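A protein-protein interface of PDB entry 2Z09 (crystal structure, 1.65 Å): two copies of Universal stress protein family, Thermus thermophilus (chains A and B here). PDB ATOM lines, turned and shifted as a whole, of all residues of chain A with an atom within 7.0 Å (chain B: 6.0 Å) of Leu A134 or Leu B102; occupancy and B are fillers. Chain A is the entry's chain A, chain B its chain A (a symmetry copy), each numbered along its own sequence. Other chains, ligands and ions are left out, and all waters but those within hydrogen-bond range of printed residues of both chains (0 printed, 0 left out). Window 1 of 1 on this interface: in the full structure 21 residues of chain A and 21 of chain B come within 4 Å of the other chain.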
ATOM      1  N   PHE A   2      10.809  -5.473  -0.851  1.00  0.00           N
ATOM      2  CA  PHE A   2      10.698  -6.058   0.480  1.00  0.00           C
ATOM      3  C   PHE A   2       9.237  -6.279   0.879  1.00  0.00           C
ATOM      4  O   PHE A   2       8.513  -5.323   1.238  1.00  0.00           O
ATOM      5  CB  PHE A   2      11.421  -5.163   1.512  1.00  0.00           C
ATOM      6  CG  PHE A   2      12.924  -4.981   1.281  1.00  0.00           C
ATOM      7  CD1 PHE A   2      13.532  -3.788   1.705  1.00  0.00           C
ATOM      8  CD2 PHE A   2      13.699  -5.996   0.677  1.00  0.00           C
ATOM      9  CE1 PHE A   2      14.847  -3.568   1.541  1.00  0.00           C
ATOM     10  CE2 PHE A   2      15.064  -5.815   0.488  1.00  0.00           C
ATOM     11  CZ  PHE A   2      15.670  -4.560   0.919  1.00  0.00           C
ATOM     12  N   ALA A  18      18.034  -3.018  16.277  1.00  0.00           N
ATOM     13  CA  ALA A  18      17.610  -3.690  15.052  1.00  0.00           C
ATOM     14  C   ALA A  18      16.076  -3.840  14.963  1.00  0.00           C
ATOM     15  O   ALA A  18      15.529  -3.772  13.872  1.00  0.00           O
ATOM     16  CB  ALA A  18      18.302  -5.165  14.938  1.00  0.00           C
ATOM     17  N   VAL A  21      14.685  -0.601  13.763  1.00  0.00           N
ATOM     18  CA  VAL A  21      14.909  -0.477  12.351  1.00  0.00           C
ATOM     19  C   VAL A  21      13.983  -1.367  11.544  1.00  0.00           C
ATOM     20  O   VAL A  21      13.474  -0.957  10.510  1.00  0.00           O
ATOM     21  CB  VAL A  21      16.401  -0.841  12.048  1.00  0.00           C
ATOM     22  CG1 VAL A  21      16.571  -1.047  10.513  1.00  0.00           C
ATOM     23  CG2 VAL A  21      17.298   0.211  12.618  1.00  0.00           C
ATOM     24  N   ALA A  22      13.722  -2.586  12.019  1.00  0.00           N
ATOM     25  CA  ALA A  22      12.908  -3.529  11.268  1.00  0.00           C
ATOM     26  C   ALA A  22      11.457  -3.061  11.244  1.00  0.00           C
ATOM     27  O   ALA A  22      10.802  -3.239  10.233  1.00  0.00           O
ATOM     28  CB  ALA A  22      13.026  -5.015  11.864  1.00  0.00           C
ATOM     29  N   GLU A  25      11.334  -0.285   8.705  1.00  0.00           N
ATOM     30  CA  GLU A  25      11.408  -0.813   7.346  1.00  0.00           C
ATOM     31  C   GLU A  25      10.070  -1.451   6.966  1.00  0.00           C
ATOM     32  O   GLU A  25       9.616  -1.284   5.885  1.00  0.00           O
ATOM     33  CB  GLU A  25      12.496  -1.925   7.226  1.00  0.00           C
ATOM     34  CG  GLU A  25      13.880  -1.481   7.273  1.00  0.00           C
ATOM     35  CD  GLU A  25      14.305  -0.778   5.988  1.00  0.00           C
ATOM     36  OE1 GLU A  25      13.457  -0.257   5.247  1.00  0.00           O
ATOM     37  OE2 GLU A  25      15.512  -0.768   5.715  1.00  0.00           O
ATOM     38  N   LEU A 102      14.323  -9.687   3.320  1.00  0.00           N
ATOM     39  CA  LEU A 102      15.336  -8.862   4.020  1.00  0.00           C
ATOM     40  C   LEU A 102      15.426  -9.462   5.439  1.00  0.00           C
ATOM     41  O   LEU A 102      14.367  -9.863   5.999  1.00  0.00           O
ATOM     42  CB  LEU A 102      14.810  -7.401   4.125  1.00  0.00           C
ATOM     43  CG  LEU A 102      15.738  -6.513   4.961  1.00  0.00           C
ATOM     44  CD1 LEU A 102      17.030  -6.353   4.196  1.00  0.00           C
ATOM     45  CD2 LEU A 102      15.137  -5.181   5.281  1.00  0.00           C
ATOM     46  N   ILE A 103      16.658  -9.664   5.922  1.00  0.00           N
ATOM     47  CA  ILE A 103      16.872 -10.091   7.299  1.00  0.00           C
ATOM     48  C   ILE A 103      17.528  -8.901   7.978  1.00  0.00           C
ATOM     49  O   ILE A 103      18.434  -8.334   7.371  1.00  0.00           O
ATOM     50  CB  ILE A 103      17.855 -11.262   7.356  1.00  0.00           C
ATOM     51  CG1 ILE A 103      17.184 -12.472   6.763  1.00  0.00           C
ATOM     52  CG2 ILE A 103      18.352 -11.464   8.834  1.00  0.00           C
ATOM     53  CD1 ILE A 103      18.264 -13.557   6.405  1.00  0.00           C
ATOM     54  N   VAL A 104      17.022  -8.493   9.157  1.00  0.00           N
ATOM     55  CA  VAL A 104      17.603  -7.349   9.896  1.00  0.00           C
ATOM     56  C   VAL A 104      18.187  -7.990  11.196  1.00  0.00           C
ATOM     57  O   VAL A 104      17.528  -8.804  11.842  1.00  0.00           O
ATOM     58  CB  VAL A 104      16.486  -6.354  10.283  1.00  0.00           C
ATOM     59  CG1 VAL A 104      17.029  -5.175  11.035  1.00  0.00           C
ATOM     60  CG2 VAL A 104      15.791  -5.865   8.988  1.00  0.00           C
ATOM     61  N   MET A 105      19.494  -7.718  11.503  1.00  0.00           N
ATOM     62  CA  MET A 105      19.989  -8.275  12.758  1.00  0.00           C
ATOM     63  C   MET A 105      21.075  -7.340  13.256  1.00  0.00           C
ATOM     64  O   MET A 105      21.504  -6.437  12.490  1.00  0.00           O
ATOM     65  CB  MET A 105      20.573  -9.723  12.539  1.00  0.00           C
ATOM     66  CG  MET A 105      21.741  -9.697  11.528  1.00  0.00           C
ATOM     67  SD  MET A 105      22.052 -11.418  10.876  1.00  0.00           S
ATOM     68  CE  MET A 105      22.302 -12.362  12.440  1.00  0.00           C
ATOM     69  N   GLY A 106      21.469  -7.501  14.534  1.00  0.00           N
ATOM     70  CA  GLY A 106      22.549  -6.613  15.008  1.00  0.00           C
ATOM     71  C   GLY A 106      23.951  -7.064  14.454  1.00  0.00           C
ATOM     72  O   GLY A 106      24.176  -8.231  14.003  1.00  0.00           O
ATOM     73  N   THR A 107      24.871  -6.098  14.472  1.00  0.00           N
ATOM     74  CA  THR A 107      26.262  -6.478  14.104  1.00  0.00           C
ATOM     75  C   THR A 107      26.841  -7.334  15.227  1.00  0.00           C
ATOM     76  O   THR A 107      27.690  -8.183  14.977  1.00  0.00           O
ATOM     77  CB  THR A 107      27.140  -5.237  13.969  1.00  0.00           C
ATOM     78  OG1 THR A 107      26.983  -4.433  15.145  1.00  0.00           O
ATOM     79  CG2 THR A 107      26.746  -4.417  12.779  1.00  0.00           C
ATOM     80  N   CYS A 131      18.860 -13.543   0.875  1.00  0.00           N
ATOM     81  CA  CYS A 131      18.381 -12.190   0.513  1.00  0.00           C
ATOM     82  C   CYS A 131      19.331 -11.172   1.200  1.00  0.00           C
ATOM     83  O   CYS A 131      20.212 -11.584   1.907  1.00  0.00           O
ATOM     84  CB  CYS A 131      16.968 -11.965   1.145  1.00  0.00           C
ATOM     85  SG  CYS A 131      16.951 -12.287   2.995  1.00  0.00           S
ATOM     86  N   PRO A 132      19.093  -9.865   1.021  1.00  0.00           N
ATOM     87  CA  PRO A 132      19.920  -8.824   1.629  1.00  0.00           C
ATOM     88  C   PRO A 132      19.818  -8.889   3.140  1.00  0.00           C
ATOM     89  O   PRO A 132      18.801  -9.359   3.727  1.00  0.00           O
ATOM     90  CB  PRO A 132      19.352  -7.491   1.115  1.00  0.00           C
ATOM     91  CG  PRO A 132      18.783  -7.879  -0.219  1.00  0.00           C
ATOM     92  CD  PRO A 132      18.158  -9.294   0.013  1.00  0.00           C
ATOM     93  N   VAL A 133      20.915  -8.452   3.796  1.00  0.00           N
ATOM     94  CA  VAL A 133      20.901  -8.514   5.283  1.00  0.00           C
ATOM     95  C   VAL A 133      21.250  -7.080   5.744  1.00  0.00           C
ATOM     96  O   VAL A 133      22.201  -6.545   5.241  1.00  0.00           O
ATOM     97  CB  VAL A 133      22.058  -9.415   5.778  1.00  0.00           C
ATOM     98  CG1 VAL A 133      22.160  -9.315   7.299  1.00  0.00           C
ATOM     99  CG2 VAL A 133      21.759 -10.920   5.320  1.00  0.00           C
ATOM    100  N   LEU A 134      20.429  -6.506   6.629  1.00  0.00           N
ATOM    101  CA  LEU A 134      20.642  -5.147   7.155  1.00  0.00           C
ATOM    102  C   LEU A 134      21.227  -5.298   8.534  1.00  0.00           C
ATOM    103  O   LEU A 134      20.571  -5.840   9.456  1.00  0.00           O
ATOM    104  CB  LEU A 134      19.257  -4.435   7.206  1.00  0.00           C
ATOM    105  CG  LEU A 134      19.183  -3.074   7.869  1.00  0.00           C
ATOM    106  CD1 LEU A 134      20.278  -2.225   7.433  1.00  0.00           C
ATOM    107  CD2 LEU A 134      17.828  -2.478   7.454  1.00  0.00           C
ATOM    108  N   LEU A 135      22.531  -4.937   8.657  1.00  0.00           N
ATOM    109  CA  LEU A 135      23.291  -5.012   9.890  1.00  0.00           C
ATOM    110  C   LEU A 135      23.167  -3.741  10.674  1.00  0.00           C
ATOM    111  O   LEU A 135      23.550  -2.682  10.210  1.00  0.00           O
ATOM    112  CB  LEU A 135      24.772  -5.345   9.552  1.00  0.00           C
ATOM    113  CG  LEU A 135      24.904  -6.745   8.961  1.00  0.00           C
ATOM    114  CD1 LEU A 135      26.406  -6.796   8.583  1.00  0.00           C
ATOM    115  CD2 LEU A 135      24.568  -7.904   9.980  1.00  0.00           C
ATOM    116  N   VAL A 136      22.688  -3.851  11.907  1.00  0.00           N
ATOM    117  CA  VAL A 136      22.413  -2.666  12.806  1.00  0.00           C
ATOM    118  C   VAL A 136      23.360  -2.610  13.956  1.00  0.00           C
ATOM    119  O   VAL A 136      23.522  -3.523  14.680  1.00  0.00           O
ATOM    120  CB  VAL A 136      20.919  -2.738  13.299  1.00  0.00           C
ATOM    121  CG1 VAL A 136      20.599  -1.581  14.254  1.00  0.00           C
ATOM    122  CG2 VAL A 136      19.968  -2.642  12.125  1.00  0.00           C
ATOM    123  N   PHE B   2      15.936   6.889   8.312  1.00  0.00           N
ATOM    124  CA  PHE B   2      16.817   7.023   7.159  1.00  0.00           C
ATOM    125  C   PHE B   2      16.501   8.284   6.351  1.00  0.00           C
ATOM    126  O   PHE B   2      15.504   8.335   5.596  1.00  0.00           O
ATOM    127  CB  PHE B   2      16.720   5.762   6.271  1.00  0.00           C
ATOM    128  CG  PHE B   2      17.142   4.452   6.944  1.00  0.00           C
ATOM    129  CD1 PHE B   2      16.545   3.254   6.523  1.00  0.00           C
ATOM    130  CD2 PHE B   2      18.130   4.436   7.955  1.00  0.00           C
ATOM    131  CE1 PHE B   2      16.875   2.070   7.066  1.00  0.00           C
ATOM    132  CE2 PHE B   2      18.507   3.235   8.544  1.00  0.00           C
ATOM    133  CZ  PHE B   2      17.859   2.005   8.103  1.00  0.00           C
ATOM    134  N   THR B   4      19.230  10.117   4.888  1.00  0.00           N
ATOM    135  CA  THR B   4      20.325  10.155   3.917  1.00  0.00           C
ATOM    136  C   THR B   4      20.865   8.741   3.796  1.00  0.00           C
ATOM    137  O   THR B   4      21.263   8.141   4.806  1.00  0.00           O
ATOM    138  CB  THR B   4      21.430  11.042   4.427  1.00  0.00           C
ATOM    139  OG1 THR B   4      20.857  12.358   4.721  1.00  0.00           O
ATOM    140  CG2 THR B   4      22.539  11.143   3.403  1.00  0.00           C
ATOM    141  N   ILE B   5      20.931   8.283   2.537  1.00  0.00           N
ATOM    142  CA  ILE B   5      21.379   6.904   2.215  1.00  0.00           C
ATOM    143  C   ILE B   5      22.575   6.998   1.327  1.00  0.00           C
ATOM    144  O   ILE B   5      22.559   7.793   0.376  1.00  0.00           O
ATOM    145  CB  ILE B   5      20.278   6.140   1.498  1.00  0.00           C
ATOM    146  CG1 ILE B   5      18.956   6.152   2.325  1.00  0.00           C
ATOM    147  CG2 ILE B   5      20.832   4.690   1.165  1.00  0.00           C
ATOM    148  CD1 ILE B   5      19.072   5.480   3.548  1.00  0.00           C
ATOM    149  N   LEU B   6      23.632   6.225   1.619  1.00  0.00           N
ATOM    150  CA  LEU B   6      24.829   6.268   0.756  1.00  0.00           C
ATOM    151  C   LEU B   6      24.986   4.921   0.104  1.00  0.00           C
ATOM    152  O   LEU B   6      25.003   3.896   0.813  1.00  0.00           O
ATOM    153  CB  LEU B   6      26.091   6.613   1.598  1.00  0.00           C
ATOM    154  CG  LEU B   6      27.335   6.798   0.707  1.00  0.00           C
ATOM    155  CD1 LEU B   6      28.113   7.932   1.326  1.00  0.00           C
ATOM    156  CD2 LEU B   6      28.185   5.532   0.489  1.00  0.00           C
ATOM    157  N   LEU B   7      25.066   4.919  -1.243  1.00  0.00           N
ATOM    158  CA  LEU B   7      25.319   3.651  -2.005  1.00  0.00           C
ATOM    159  C   LEU B   7      26.782   3.651  -2.381  1.00  0.00           C
ATOM    160  O   LEU B   7      27.284   4.630  -2.979  1.00  0.00           O
ATOM    161  CB  LEU B   7      24.452   3.705  -3.259  1.00  0.00           C
ATOM    162  CG  LEU B   7      24.936   2.649  -4.285  1.00  0.00           C
ATOM    163  CD1 LEU B   7      24.637   1.219  -3.805  1.00  0.00           C
ATOM    164  CD2 LEU B   7      24.158   2.921  -5.616  1.00  0.00           C
ATOM    165  N   GLU B  25      14.962   1.963  -1.347  1.00  0.00           N
ATOM    166  CA  GLU B  25      14.989   2.432   0.036  1.00  0.00           C
ATOM    167  C   GLU B  25      14.819   3.953   0.069  1.00  0.00           C
ATOM    168  O   GLU B  25      14.126   4.457   0.886  1.00  0.00           O
ATOM    169  CB  GLU B  25      16.354   2.108   0.720  1.00  0.00           C
ATOM    170  CG  GLU B  25      16.596   0.713   1.047  1.00  0.00           C
ATOM    171  CD  GLU B  25      15.767   0.247   2.239  1.00  0.00           C
ATOM    172  OE1 GLU B  25      14.718   0.836   2.543  1.00  0.00           O
ATOM    173  OE2 GLU B  25      16.191  -0.719   2.888  1.00  0.00           O
ATOM    174  N   ALA B 100      25.374  10.194   6.460  1.00  0.00           N
ATOM    175  CA  ALA B 100      24.544   9.022   6.063  1.00  0.00           C
ATOM    176  C   ALA B 100      23.986   8.197   7.271  1.00  0.00           C
ATOM    177  O   ALA B 100      24.645   8.009   8.302  1.00  0.00           O
ATOM    178  CB  ALA B 100      25.372   8.109   5.212  1.00  0.00           C
ATOM    179  N   ASP B 101      22.711   7.859   7.137  1.00  0.00           N
ATOM    180  CA  ASP B 101      21.950   7.060   8.132  1.00  0.00           C
ATOM    181  C   ASP B 101      21.911   5.588   7.675  1.00  0.00           C
ATOM    182  O   ASP B 101      21.464   4.717   8.494  1.00  0.00           O
ATOM    183  CB  ASP B 101      20.468   7.575   8.183  1.00  0.00           C
ATOM    184  CG  ASP B 101      20.416   9.005   8.583  1.00  0.00           C
ATOM    185  OD1 ASP B 101      19.805   9.785   7.836  1.00  0.00           O
ATOM    186  OD2 ASP B 101      21.033   9.347   9.618  1.00  0.00           O
ATOM    187  N   LEU B 102      22.368   5.281   6.430  1.00  0.00           N
ATOM    188  CA  LEU B 102      22.346   3.877   5.957  1.00  0.00           C
ATOM    189  C   LEU B 102      23.356   3.833   4.791  1.00  0.00           C
ATOM    190  O   LEU B 102      23.418   4.818   4.003  1.00  0.00           O
ATOM    191  CB  LEU B 102      20.927   3.554   5.405  1.00  0.00           C
ATOM    192  CG  LEU B 102      20.860   2.161   4.767  1.00  0.00           C
ATOM    193  CD1 LEU B 102      21.033   1.145   5.869  1.00  0.00           C
ATOM    194  CD2 LEU B 102      19.587   1.927   4.016  1.00  0.00           C
ATOM    195  N   ILE B 103      24.218   2.809   4.791  1.00  0.00           N
ATOM    196  CA  ILE B 103      25.123   2.581   3.671  1.00  0.00           C
ATOM    197  C   ILE B 103      24.633   1.294   3.030  1.00  0.00           C
ATOM    198  O   ILE B 103      24.350   0.363   3.781  1.00  0.00           O
ATOM    199  CB  ILE B 103      26.550   2.342   4.168  1.00  0.00           C
ATOM    200  CG1 ILE B 103      27.079   3.635   4.729  1.00  0.00           C
ATOM    201  CG2 ILE B 103      27.422   1.742   3.005  1.00  0.00           C
ATOM    202  CD1 ILE B 103      28.339   3.351   5.625  1.00  0.00           C
ATOM    203  N   VAL B 104      24.460   1.283   1.695  1.00  0.00           N
ATOM    204  CA  VAL B 104      23.996   0.071   0.983  1.00  0.00           C
ATOM    205  C   VAL B 104      25.215  -0.343   0.098  1.00  0.00           C
ATOM    206  O   VAL B 104      25.825   0.499  -0.559  1.00  0.00           O
ATOM    207  CB  VAL B 104      22.805   0.427   0.066  1.00  0.00           C
ATOM    208  CG1 VAL B 104      22.300  -0.774  -0.678  1.00  0.00           C
ATOM    209  CG2 VAL B 104      21.667   1.011   0.938  1.00  0.00           C
ATOM    210  N   CYS B 131      26.762   3.911  10.930  1.00  0.00           N
ATOM    211  CA  CYS B 131      25.299   3.694  10.845  1.00  0.00           C
ATOM    212  C   CYS B 131      25.084   2.246  10.327  1.00  0.00           C
ATOM    213  O   CYS B 131      26.045   1.580  10.044  1.00  0.00           O
ATOM    214  CB  CYS B 131      24.708   4.643   9.752  1.00  0.00           C
ATOM    215  SG  CYS B 131      25.580   4.464   8.099  1.00  0.00           S
ATOM    216  N   PRO B 132      23.825   1.815  10.162  1.00  0.00           N
ATOM    217  CA  PRO B 132      23.511   0.474   9.671  1.00  0.00           C
ATOM    218  C   PRO B 132      24.020   0.301   8.254  1.00  0.00           C
ATOM    219  O   PRO B 132      24.167   1.280   7.467  1.00  0.00           O
ATOM    220  CB  PRO B 132      21.978   0.371   9.702  1.00  0.00           C
ATOM    221  CG  PRO B 132      21.616   1.303  10.822  1.00  0.00           C
ATOM    222  CD  PRO B 132      22.610   2.503  10.675  1.00  0.00           C
ATOM    223  N   VAL B 133      24.345  -0.968   7.925  1.00  0.00           N
ATOM    224  CA  VAL B 133      24.881  -1.212   6.559  1.00  0.00           C
ATOM    225  C   VAL B 133      23.981  -2.323   5.970  1.00  0.00           C
ATOM    226  O   VAL B 133      23.779  -3.296   6.646  1.00  0.00           O
ATOM    227  CB  VAL B 133      26.302  -1.819   6.657  1.00  0.00           C
ATOM    228  CG1 VAL B 133      26.763  -2.250   5.265  1.00  0.00           C
ATOM    229  CG2 VAL B 133      27.283  -0.714   7.271  1.00  0.00           C
ATOM    230  N   LEU B 134      23.436  -2.098   4.771  1.00  0.00           N
ATOM    231  CA  LEU B 134      22.561  -3.070   4.093  1.00  0.00           C
ATOM    232  C   LEU B 134      23.396  -3.750   3.041  1.00  0.00           C
ATOM    233  O   LEU B 134      23.871  -3.101   2.077  1.00  0.00           O
ATOM    234  CB  LEU B 134      21.382  -2.281   3.452  1.00  0.00           C
ATOM    235  CG  LEU B 134      20.427  -3.040   2.552  1.00  0.00           C
ATOM    236  CD1 LEU B 134      20.045  -4.306   3.152  1.00  0.00           C
ATOM    237  CD2 LEU B 134      19.203  -2.126   2.374  1.00  0.00           C
ATOM    238  N   LEU B 135      23.699  -5.051   3.288  1.00  0.00           N
ATOM    239  CA  LEU B 135      24.499  -5.888   2.413  1.00  0.00           C
ATOM    240  C   LEU B 135      23.637  -6.583   1.402  1.00  0.00           C
ATOM    241  O   LEU B 135      22.761  -7.353   1.753  1.00  0.00           O
ATOM    242  CB  LEU B 135      25.308  -6.896   3.278  1.00  0.00           C
ATOM    243  CG  LEU B 135      26.344  -6.180   4.138  1.00  0.00           C
ATOM    244  CD1 LEU B 135      26.913  -7.340   4.992  1.00  0.00           C
ATOM    245  CD2 LEU B 135      27.507  -5.505   3.309  1.00  0.00           C
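The backbone carbonyl oxygen (O) of Val A133 is in hydrogen-bond range of the backbone NH (N) of Leu B135. O of Val B133 is in hydrogen-bond range of N of Leu A135 (2.9 Å). OE2 of Glu A25 lies close to OE2 of Glu B25, 2.9 Å away.
SG of Cys A131 is in hydrogen-bond range of N of Leu A102, 3.7 Å away. N of Leu A134 lies within hydrogen-bond range of O of Ile A103. The backbone carbonyl oxygen (O) of Leu A134 is in hydrogen-bond range of the backbone NH (N) of Met A105 (3.0 Å). The backbone carbonyl oxygen (O) of Leu B102 lies within hydrogen-bond range of the backbone NH (N) of Leu B6 (2.8 Å). N of Leu B102 is in hydrogen-bond range of SG of Cys B131, at 3.7 Å. N of Ile B103 is in hydrogen-bond range of O of Pro B132 (3.1 Å).
Among the printed residues, merely in contact across the chains: Pro A132 with Leu B135 (3.2 Å), Leu A135 with Pro B132 (3.2 Å), Glu A25 with Phe B2 (3.4 Å), Phe A2 with Glu B25 (3.4 Å), Leu A135 with Leu B135 (3.7 Å), Val A133 with Leu B134 (3.7 Å), Leu A134 with Val B133 (3.7 Å), Leu A102 with Leu B134 (3.8 Å), Leu A134 with Leu B102 (3.8 Å), Pro A132 with Leu B134 (3.8 Å), Leu A134 with Pro B132 (3.8 Å) and Val A133 with Val B133 (3.9 Å).
Of chain B, only Leu B102 (3.8 Å), Pro B132 (3.8 Å) and Val B133 (3.7 Å) come within 4 Å of Leu A134. Leu B102 touches just one residue of chain A: Leu A134. Printed residues of chain A within 4 Å of Leu B134: Leu A102 (3.8 Å), Pro A132 (3.8 Å) and Val A133 (3.7 Å). Printed residues of chain A within 4 Å of Phe B2: Glu A25 (3.4 Å). Of the printed residues of chain B, Pro A132 touches Leu B134 and Leu B135. Of the printed residues of chain B, Leu A102 touches Leu B134 (3.8 Å). The nearest residue of chain A that does not touch Leu B102 is Glu A25 (5.2 Å). The nearest printed residue of chain A that does not touch Leu B135 is Leu A134 (4.9 Å).
Printed residues of chain B that touch a printed residue of chain A: Phe B2, Glu B25, Leu B102, Pro B132, Val B133, Leu B134 and Leu B135. Hydrophobic or aromatic side chains of chain B that line the printed part of chain A: Phe B2, Leu B102, Pro B132, Leu B134 and Leu B135. Along chain B the printed residues that touch a printed residue of chain A span positions 2 to 135.
Pro A132 touches Leu B135, and with the chains exchanged Leu A135 touches Pro B132. Val B133 touches its own counterpart, Val A133. Val A133 touches Leu B134, and with the chains exchanged Leu A134 touches Val B133. Leu A135 touches its own counterpart, Leu B135.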
